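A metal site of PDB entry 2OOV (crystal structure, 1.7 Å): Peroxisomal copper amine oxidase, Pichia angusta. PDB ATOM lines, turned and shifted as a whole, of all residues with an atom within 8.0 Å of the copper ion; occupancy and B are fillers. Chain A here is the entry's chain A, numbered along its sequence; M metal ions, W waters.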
ATOM      1  N   VAL A 291     -15.397   3.477   6.565  1.00  0.00           N
ATOM      2  CA  VAL A 291     -15.997   2.742   7.679  1.00  0.00           C
ATOM      3  C   VAL A 291     -15.777   1.233   7.411  1.00  0.00           C
ATOM      4  O   VAL A 291     -16.686   0.519   6.979  1.00  0.00           O
ATOM      5  CB  VAL A 291     -17.493   3.077   7.820  1.00  0.00           C
ATOM      6  CG1 VAL A 291     -18.097   2.413   9.055  1.00  0.00           C
ATOM      7  CG2 VAL A 291     -17.724   4.593   7.853  1.00  0.00           C
ATOM      8  N   TYR A 293     -15.510  -2.619   7.804  1.00  0.00           N
ATOM      9  CA  TYR A 293     -15.997  -3.729   8.632  1.00  0.00           C
ATOM     10  C   TYR A 293     -14.940  -4.826   8.790  1.00  0.00           C
ATOM     11  O   TYR A 293     -14.040  -4.977   7.951  1.00  0.00           O
ATOM     12  CB  TYR A 293     -17.335  -4.252   8.060  1.00  0.00           C
ATOM     13  CG  TYR A 293     -18.468  -3.365   8.512  1.00  0.00           C
ATOM     14  CD1 TYR A 293     -18.639  -2.103   7.924  1.00  0.00           C
ATOM     15  CD2 TYR A 293     -19.335  -3.749   9.549  1.00  0.00           C
ATOM     16  CE1 TYR A 293     -19.639  -1.248   8.334  1.00  0.00           C
ATOM     17  CE2 TYR A 293     -20.366  -2.880   9.976  1.00  0.00           C
ATOM     18  CZ  TYR A 293     -20.501  -1.631   9.349  1.00  0.00           C
ATOM     19  OH  TYR A 293     -21.487  -0.743   9.723  1.00  0.00           O
ATOM     20  N   ASN A 392     -28.261   3.325   7.315  1.00  0.00           N
ATOM     21  CA  ASN A 392     -28.480   3.044   8.729  1.00  0.00           C
ATOM     22  C   ASN A 392     -27.901   4.106   9.679  1.00  0.00           C
ATOM     23  O   ASN A 392     -28.431   4.308  10.762  1.00  0.00           O
ATOM     24  CB  ASN A 392     -27.932   1.640   9.106  1.00  0.00           C
ATOM     25  CG  ASN A 392     -26.479   1.459   8.729  1.00  0.00           C
ATOM     26  OD1 ASN A 392     -26.138   1.460   7.547  1.00  0.00           O
ATOM     27  ND2 ASN A 392     -25.604   1.327   9.724  1.00  0.00           N
ATOM     28  N   TPQ A 393     -26.828   4.722   9.413  1.00  0.00           N
ATOM     29  CA  TPQ A 393     -25.965   5.539  10.274  1.00  0.00           C
ATOM     30  CB  TPQ A 393     -24.540   5.669   9.731  1.00  0.00           C
ATOM     31  C   TPQ A 393     -26.507   6.946  10.319  1.00  0.00           C
ATOM     32  O   TPQ A 393     -26.771   7.489   9.218  1.00  0.00           O
ATOM     33  C1  TPQ A 393     -23.884   4.380   9.298  1.00  0.00           C
ATOM     34  C2  TPQ A 393     -23.141   3.542  10.285  1.00  0.00           C
ATOM     35  O2  TPQ A 393     -23.061   3.931  11.585  1.00  0.00           O
ATOM     36  C3  TPQ A 393     -22.533   2.355   9.911  1.00  0.00           C
ATOM     37  C4  TPQ A 393     -22.628   1.952   8.584  1.00  0.00           C
ATOM     38  O4  TPQ A 393     -22.036   0.802   8.181  1.00  0.00           O
ATOM     39  C5  TPQ A 393     -23.383   2.777   7.581  1.00  0.00           C
ATOM     40  O5  TPQ A 393     -23.466   2.356   6.283  1.00  0.00           O
ATOM     41  C6  TPQ A 393     -23.976   3.968   7.972  1.00  0.00           C
ATOM     42  N   TYR A 395     -24.581  10.702  11.371  1.00  0.00           N
ATOM     43  CA  TYR A 395     -23.375  11.421  11.768  1.00  0.00           C
ATOM     44  C   TYR A 395     -23.792  12.845  12.060  1.00  0.00           C
ATOM     45  O   TYR A 395     -24.270  13.557  11.169  1.00  0.00           O
ATOM     46  CB  TYR A 395     -22.324  11.395  10.647  1.00  0.00           C
ATOM     47  CG  TYR A 395     -21.790  10.027  10.364  1.00  0.00           C
ATOM     48  CD1 TYR A 395     -22.390   9.196   9.406  1.00  0.00           C
ATOM     49  CD2 TYR A 395     -20.698   9.533  11.077  1.00  0.00           C
ATOM     50  CE1 TYR A 395     -21.887   7.914   9.157  1.00  0.00           C
ATOM     51  CE2 TYR A 395     -20.198   8.261  10.828  1.00  0.00           C
ATOM     52  CZ  TYR A 395     -20.792   7.462   9.878  1.00  0.00           C
ATOM     53  OH  TYR A 395     -20.263   6.216   9.640  1.00  0.00           O
ATOM     54  N   LEU A 413     -21.933   9.968  16.829  1.00  0.00           N
ATOM     55  CA  LEU A 413     -22.417   8.855  16.034  1.00  0.00           C
ATOM     56  C   LEU A 413     -23.701   8.296  16.629  1.00  0.00           C
ATOM     57  O   LEU A 413     -23.757   7.958  17.809  1.00  0.00           O
ATOM     58  CB  LEU A 413     -21.391   7.720  16.006  1.00  0.00           C
ATOM     59  CG  LEU A 413     -19.960   7.995  15.566  1.00  0.00           C
ATOM     60  CD1 LEU A 413     -19.210   6.665  15.454  1.00  0.00           C
ATOM     61  CD2 LEU A 413     -19.928   8.696  14.237  1.00  0.00           C
ATOM     62  N   THR A 414     -24.733   8.189  15.801  1.00  0.00           N
ATOM     63  CA  THR A 414     -25.975   7.566  16.223  1.00  0.00           C
ATOM     64  C   THR A 414     -26.596   6.812  15.050  1.00  0.00           C
ATOM     65  O   THR A 414     -25.886   6.404  14.119  1.00  0.00           O
ATOM     66  CB  THR A 414     -26.932   8.575  16.965  1.00  0.00           C
ATOM     67  OG1 THR A 414     -28.071   7.873  17.510  1.00  0.00           O
ATOM     68  CG2 THR A 414     -27.405   9.687  16.069  1.00  0.00           C
ATOM     69  N   ILE A 416     -28.497   3.459  13.431  1.00  0.00           N
ATOM     70  CA  ILE A 416     -28.685   2.025  13.644  1.00  0.00           C
ATOM     71  C   ILE A 416     -27.460   1.220  13.205  1.00  0.00           C
ATOM     72  O   ILE A 416     -26.839   1.540  12.183  1.00  0.00           O
ATOM     73  CB  ILE A 416     -29.975   1.564  12.943  1.00  0.00           C
ATOM     74  CG1 ILE A 416     -31.147   2.392  13.522  1.00  0.00           C
ATOM     75  CG2 ILE A 416     -30.190   0.042  13.137  1.00  0.00           C
ATOM     76  CD1 ILE A 416     -32.509   2.058  12.976  1.00  0.00           C
ATOM     77  N   LEU A 417     -27.111   0.203  13.992  1.00  0.00           N
ATOM     78  CA  LEU A 417     -26.075  -0.757  13.590  1.00  0.00           C
ATOM     79  C   LEU A 417     -26.379  -1.400  12.227  1.00  0.00           C
ATOM     80  O   LEU A 417     -27.512  -1.805  11.968  1.00  0.00           O
ATOM     81  CB  LEU A 417     -25.974  -1.879  14.631  1.00  0.00           C
ATOM     82  CG  LEU A 417     -25.462  -1.518  16.020  1.00  0.00           C
ATOM     83  CD1 LEU A 417     -25.705  -2.707  16.946  1.00  0.00           C
ATOM     84  CD2 LEU A 417     -23.976  -1.117  15.973  1.00  0.00           C
ATOM     85  N   ASN A 418     -25.360  -1.494  11.365  1.00  0.00           N
ATOM     86  CA  ASN A 418     -25.512  -2.380  10.215  1.00  0.00           C
ATOM     87  C   ASN A 418     -25.541  -3.788  10.769  1.00  0.00           C
ATOM     88  O   ASN A 418     -24.739  -4.121  11.639  1.00  0.00           O
ATOM     89  CB  ASN A 418     -24.374  -2.233   9.206  1.00  0.00           C
ATOM     90  CG  ASN A 418     -24.274  -3.431   8.269  1.00  0.00           C
ATOM     91  OD1 ASN A 418     -23.593  -4.417   8.577  1.00  0.00           O
ATOM     92  ND2 ASN A 418     -24.984  -3.365   7.163  1.00  0.00           N
ATOM     93  N   HIS A 442     -21.609  -6.663  12.906  1.00  0.00           N
ATOM     94  CA  HIS A 442     -20.169  -6.805  12.674  1.00  0.00           C
ATOM     95  C   HIS A 442     -19.358  -5.642  13.229  1.00  0.00           C
ATOM     96  O   HIS A 442     -19.807  -4.491  13.213  1.00  0.00           O
ATOM     97  CB  HIS A 442     -19.881  -6.898  11.171  1.00  0.00           C
ATOM     98  CG  HIS A 442     -20.374  -8.166  10.532  1.00  0.00           C
ATOM     99  ND1 HIS A 442     -20.767  -8.215   9.209  1.00  0.00           N
ATOM    100  CD2 HIS A 442     -20.530  -9.418  11.016  1.00  0.00           C
ATOM    101  CE1 HIS A 442     -21.125  -9.452   8.906  1.00  0.00           C
ATOM    102  NE2 HIS A 442     -20.990 -10.198   9.989  1.00  0.00           N
ATOM    103  N   ASN A 443     -18.140  -5.976  13.673  1.00  0.00           N
ATOM    104  CA  ASN A 443     -17.162  -4.980  14.081  1.00  0.00           C
ATOM    105  C   ASN A 443     -16.849  -4.063  12.916  1.00  0.00           C
ATOM    106  O   ASN A 443     -16.825  -4.510  11.758  1.00  0.00           O
ATOM    107  CB  ASN A 443     -15.857  -5.663  14.483  1.00  0.00           C
ATOM    108  CG  ASN A 443     -16.023  -6.630  15.645  1.00  0.00           C
ATOM    109  OD1 ASN A 443     -17.006  -6.569  16.376  1.00  0.00           O
ATOM    110  ND2 ASN A 443     -15.028  -7.505  15.837  1.00  0.00           N
ATOM    111  N   HIS A 444     -16.566  -2.791  13.205  1.00  0.00           N
ATOM    112  CA  HIS A 444     -16.183  -1.848  12.165  1.00  0.00           C
ATOM    113  C   HIS A 444     -15.500  -0.641  12.790  1.00  0.00           C
ATOM    114  O   HIS A 444     -15.671  -0.359  13.974  1.00  0.00           O
ATOM    115  CB  HIS A 444     -17.423  -1.397  11.378  1.00  0.00           C
ATOM    116  CG  HIS A 444     -18.469  -0.787  12.247  1.00  0.00           C
ATOM    117  ND1 HIS A 444     -19.336  -1.551  13.007  1.00  0.00           N
ATOM    118  CD2 HIS A 444     -18.768   0.510  12.517  1.00  0.00           C
ATOM    119  CE1 HIS A 444     -20.123  -0.740  13.706  1.00  0.00           C
ATOM    120  NE2 HIS A 444     -19.798   0.509  13.418  1.00  0.00           N
ATOM    121  N   GLN A 445     -14.733   0.080  11.976  1.00  0.00           N
ATOM    122  CA  GLN A 445     -14.141   1.349  12.393  1.00  0.00           C
ATOM    123  C   GLN A 445     -14.897   2.471  11.673  1.00  0.00           C
ATOM    124  O   GLN A 445     -15.441   2.246  10.594  1.00  0.00           O
ATOM    125  CB  GLN A 445     -12.664   1.419  11.996  1.00  0.00           C
ATOM    126  CG  GLN A 445     -11.800   0.321  12.626  1.00  0.00           C
ATOM    127  CD  GLN A 445     -10.311   0.568  12.421  1.00  0.00           C
ATOM    128  OE1 GLN A 445      -9.767   0.246  11.373  1.00  0.00           O
ATOM    129  NE2 GLN A 445      -9.664   1.143  13.423  1.00  0.00           N
ATOM    130  N   HIS A 446     -14.937   3.662  12.275  1.00  0.00           N
ATOM    131  CA  HIS A 446     -15.359   4.867  11.568  1.00  0.00           C
ATOM    132  C   HIS A 446     -14.159   5.809  11.530  1.00  0.00           C
ATOM    133  O   HIS A 446     -13.747   6.301  12.575  1.00  0.00           O
ATOM    134  CB  HIS A 446     -16.496   5.590  12.309  1.00  0.00           C
ATOM    135  CG  HIS A 446     -17.723   4.766  12.543  1.00  0.00           C
ATOM    136  ND1 HIS A 446     -18.873   4.930  11.812  1.00  0.00           N
ATOM    137  CD2 HIS A 446     -18.016   3.863  13.517  1.00  0.00           C
ATOM    138  CE1 HIS A 446     -19.817   4.118  12.284  1.00  0.00           C
ATOM    139  NE2 HIS A 446     -19.310   3.464  13.330  1.00  0.00           N
ATOM    140  N   ILE A 610     -13.113   6.192  15.510  1.00  0.00           N
ATOM    141  CA  ILE A 610     -13.294   5.211  16.563  1.00  0.00           C
ATOM    142  C   ILE A 610     -13.313   3.803  15.999  1.00  0.00           C
ATOM    143  O   ILE A 610     -13.503   3.594  14.788  1.00  0.00           O
ATOM    144  CB  ILE A 610     -14.596   5.447  17.354  1.00  0.00           C
ATOM    145  CG1 ILE A 610     -15.810   5.330  16.428  1.00  0.00           C
ATOM    146  CG2 ILE A 610     -14.567   6.797  18.105  1.00  0.00           C
ATOM    147  CD1 ILE A 610     -17.005   4.739  17.095  1.00  0.00           C
ATOM    148  N   THR A 611     -13.125   2.832  16.896  1.00  0.00           N
ATOM    149  CA  THR A 611     -13.267   1.428  16.548  1.00  0.00           C
ATOM    150  C   THR A 611     -14.470   0.927  17.336  1.00  0.00           C
ATOM    151  O   THR A 611     -14.489   1.008  18.566  1.00  0.00           O
ATOM    152  CB  THR A 611     -11.995   0.634  16.893  1.00  0.00           C
ATOM    153  OG1 THR A 611     -10.908   1.160  16.123  1.00  0.00           O
ATOM    154  CG2 THR A 611     -12.183  -0.862  16.572  1.00  0.00           C
ATOM    155  N   HIS A 612     -15.492   0.464  16.609  1.00  0.00           N
ATOM    156  CA  HIS A 612     -16.766   0.091  17.200  1.00  0.00           C
ATOM    157  C   HIS A 612     -16.902  -1.444  17.323  1.00  0.00           C
ATOM    158  O   HIS A 612     -16.929  -2.148  16.317  1.00  0.00           O
ATOM    159  CB  HIS A 612     -17.877   0.653  16.312  1.00  0.00           C
ATOM    160  CG  HIS A 612     -19.247   0.607  16.930  1.00  0.00           C
ATOM    161  ND1 HIS A 612     -20.326   1.248  16.349  1.00  0.00           N
ATOM    162  CD2 HIS A 612     -19.705   0.006  18.051  1.00  0.00           C
ATOM    163  CE1 HIS A 612     -21.392   1.044  17.105  1.00  0.00           C
ATOM    164  NE2 HIS A 612     -21.047   0.293  18.136  1.00  0.00           N
ATOM    165  N   PHE A 613     -16.951  -1.934  18.563  1.00  0.00           N
ATOM    166  CA  PHE A 613     -17.328  -3.328  18.852  1.00  0.00           C
ATOM    167  C   PHE A 613     -18.747  -3.272  19.414  1.00  0.00           C
ATOM    168  O   PHE A 613     -18.949  -2.884  20.569  1.00  0.00           O
ATOM    169  CB  PHE A 613     -16.351  -3.929  19.880  1.00  0.00           C
ATOM    170  CG  PHE A 613     -14.935  -4.006  19.371  1.00  0.00           C
ATOM    171  CD1 PHE A 613     -14.578  -4.973  18.438  1.00  0.00           C
ATOM    172  CD2 PHE A 613     -13.978  -3.086  19.799  1.00  0.00           C
ATOM    173  CE1 PHE A 613     -13.278  -5.045  17.938  1.00  0.00           C
ATOM    174  CE2 PHE A 613     -12.674  -3.147  19.318  1.00  0.00           C
ATOM    175  CZ  PHE A 613     -12.329  -4.127  18.368  1.00  0.00           C
ATOM    176  N   PRO A 614     -19.762  -3.580  18.562  1.00  0.00           N
ATOM    177  CA  PRO A 614     -21.153  -3.416  18.998  1.00  0.00           C
ATOM    178  C   PRO A 614     -21.509  -4.168  20.299  1.00  0.00           C
ATOM    179  O   PRO A 614     -20.962  -5.235  20.594  1.00  0.00           O
ATOM    180  CB  PRO A 614     -21.963  -3.956  17.808  1.00  0.00           C
ATOM    181  CG  PRO A 614     -21.051  -3.736  16.604  1.00  0.00           C
ATOM    182  CD  PRO A 614     -19.662  -4.042  17.159  1.00  0.00           C
ATOM    183  N   ASP A 618     -26.344  -0.697  21.950  1.00  0.00           N
ATOM    184  CA  ASP A 618     -26.368   0.022  20.664  1.00  0.00           C
ATOM    185  C   ASP A 618     -27.616  -0.307  19.832  1.00  0.00           C
ATOM    186  O   ASP A 618     -27.821   0.280  18.754  1.00  0.00           O
ATOM    187  CB  ASP A 618     -25.147  -0.355  19.809  1.00  0.00           C
ATOM    188  CG  ASP A 618     -23.816   0.002  20.454  1.00  0.00           C
ATOM    189  OD1 ASP A 618     -23.779   0.975  21.246  1.00  0.00           O
ATOM    190  OD2 ASP A 618     -22.812  -0.698  20.148  1.00  0.00           O
ATOM    191  N   SME A 622     -28.939   3.299  18.407  1.00  0.00           N
ATOM    192  CA  SME A 622     -27.785   3.485  19.283  1.00  0.00           C
ATOM    193  CB  SME A 622     -26.538   3.093  18.474  1.00  0.00           C
ATOM    194  CG  SME A 622     -25.950   4.257  17.710  1.00  0.00           C
ATOM    195  S   SME A 622     -24.432   3.638  16.897  1.00  0.00           S
ATOM    196  OE  SME A 622     -25.024   2.675  15.460  1.00  0.00           O
ATOM    197  CE  SME A 622     -23.742   2.811  18.289  1.00  0.00           C
ATOM    198  C   SME A 622     -27.641   4.849  19.921  1.00  0.00           C
ATOM    199  O   SME A 622     -27.765   5.855  19.254  1.00  0.00           O
ATOM    200  N   GLU A 625     -22.445   8.284  20.352  1.00  0.00           N
ATOM    201  CA  GLU A 625     -21.055   8.101  20.775  1.00  0.00           C
ATOM    202  C   GLU A 625     -20.221   9.298  20.288  1.00  0.00           C
ATOM    203  O   GLU A 625     -20.223   9.582  19.084  1.00  0.00           O
ATOM    204  CB  GLU A 625     -20.468   6.806  20.195  1.00  0.00           C
ATOM    205  CG  GLU A 625     -19.033   6.571  20.704  1.00  0.00           C
ATOM    206  CD  GLU A 625     -18.422   5.272  20.211  1.00  0.00           C
ATOM    207  OE1 GLU A 625     -19.119   4.512  19.502  1.00  0.00           O
ATOM    208  OE2 GLU A 625     -17.212   5.028  20.498  1.00  0.00           O
HETATM  209 CU    CU M   1     -20.195   2.123  14.540  1.00  0.00          CU
HETATM  210  O   HOH W   1     -22.656   1.741  13.480  1.00  0.00           O
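The backbone carbonyl oxygen (O) of His 442 lies within hydrogen-bond range of a ring nitrogen (ND1) of His 444 (3.0 Å).
N of His 446 is in hydrogen-bond range of O of Ile 610 (2.9 Å).
The side-chain hydroxyl (OH) of Tyr 395 lies within hydrogen-bond range of a ring nitrogen (ND1) of His 446 (2.9 Å).
A ring nitrogen (NE2) of His 612 lies within hydrogen-bond range of the side-chain carboxylate of Asp 618 (2.9 Å).
Of the 23 residues printed, 3 come within 4 Å of the copper ion.
The copper ion is bound by NE2 of His 444 (2.0 Å).
The copper ion is bound by NE2 of His 446 (2.0 Å).
The copper ion is bound by ND1 of His 612 (2.0 Å).
Slightly farther from the copper ion lies water W1 (2.7 Å).
Water W1 bridges O2 of TPQ 393 (2.9 Å) and OE of SME 622 (3.2 Å).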
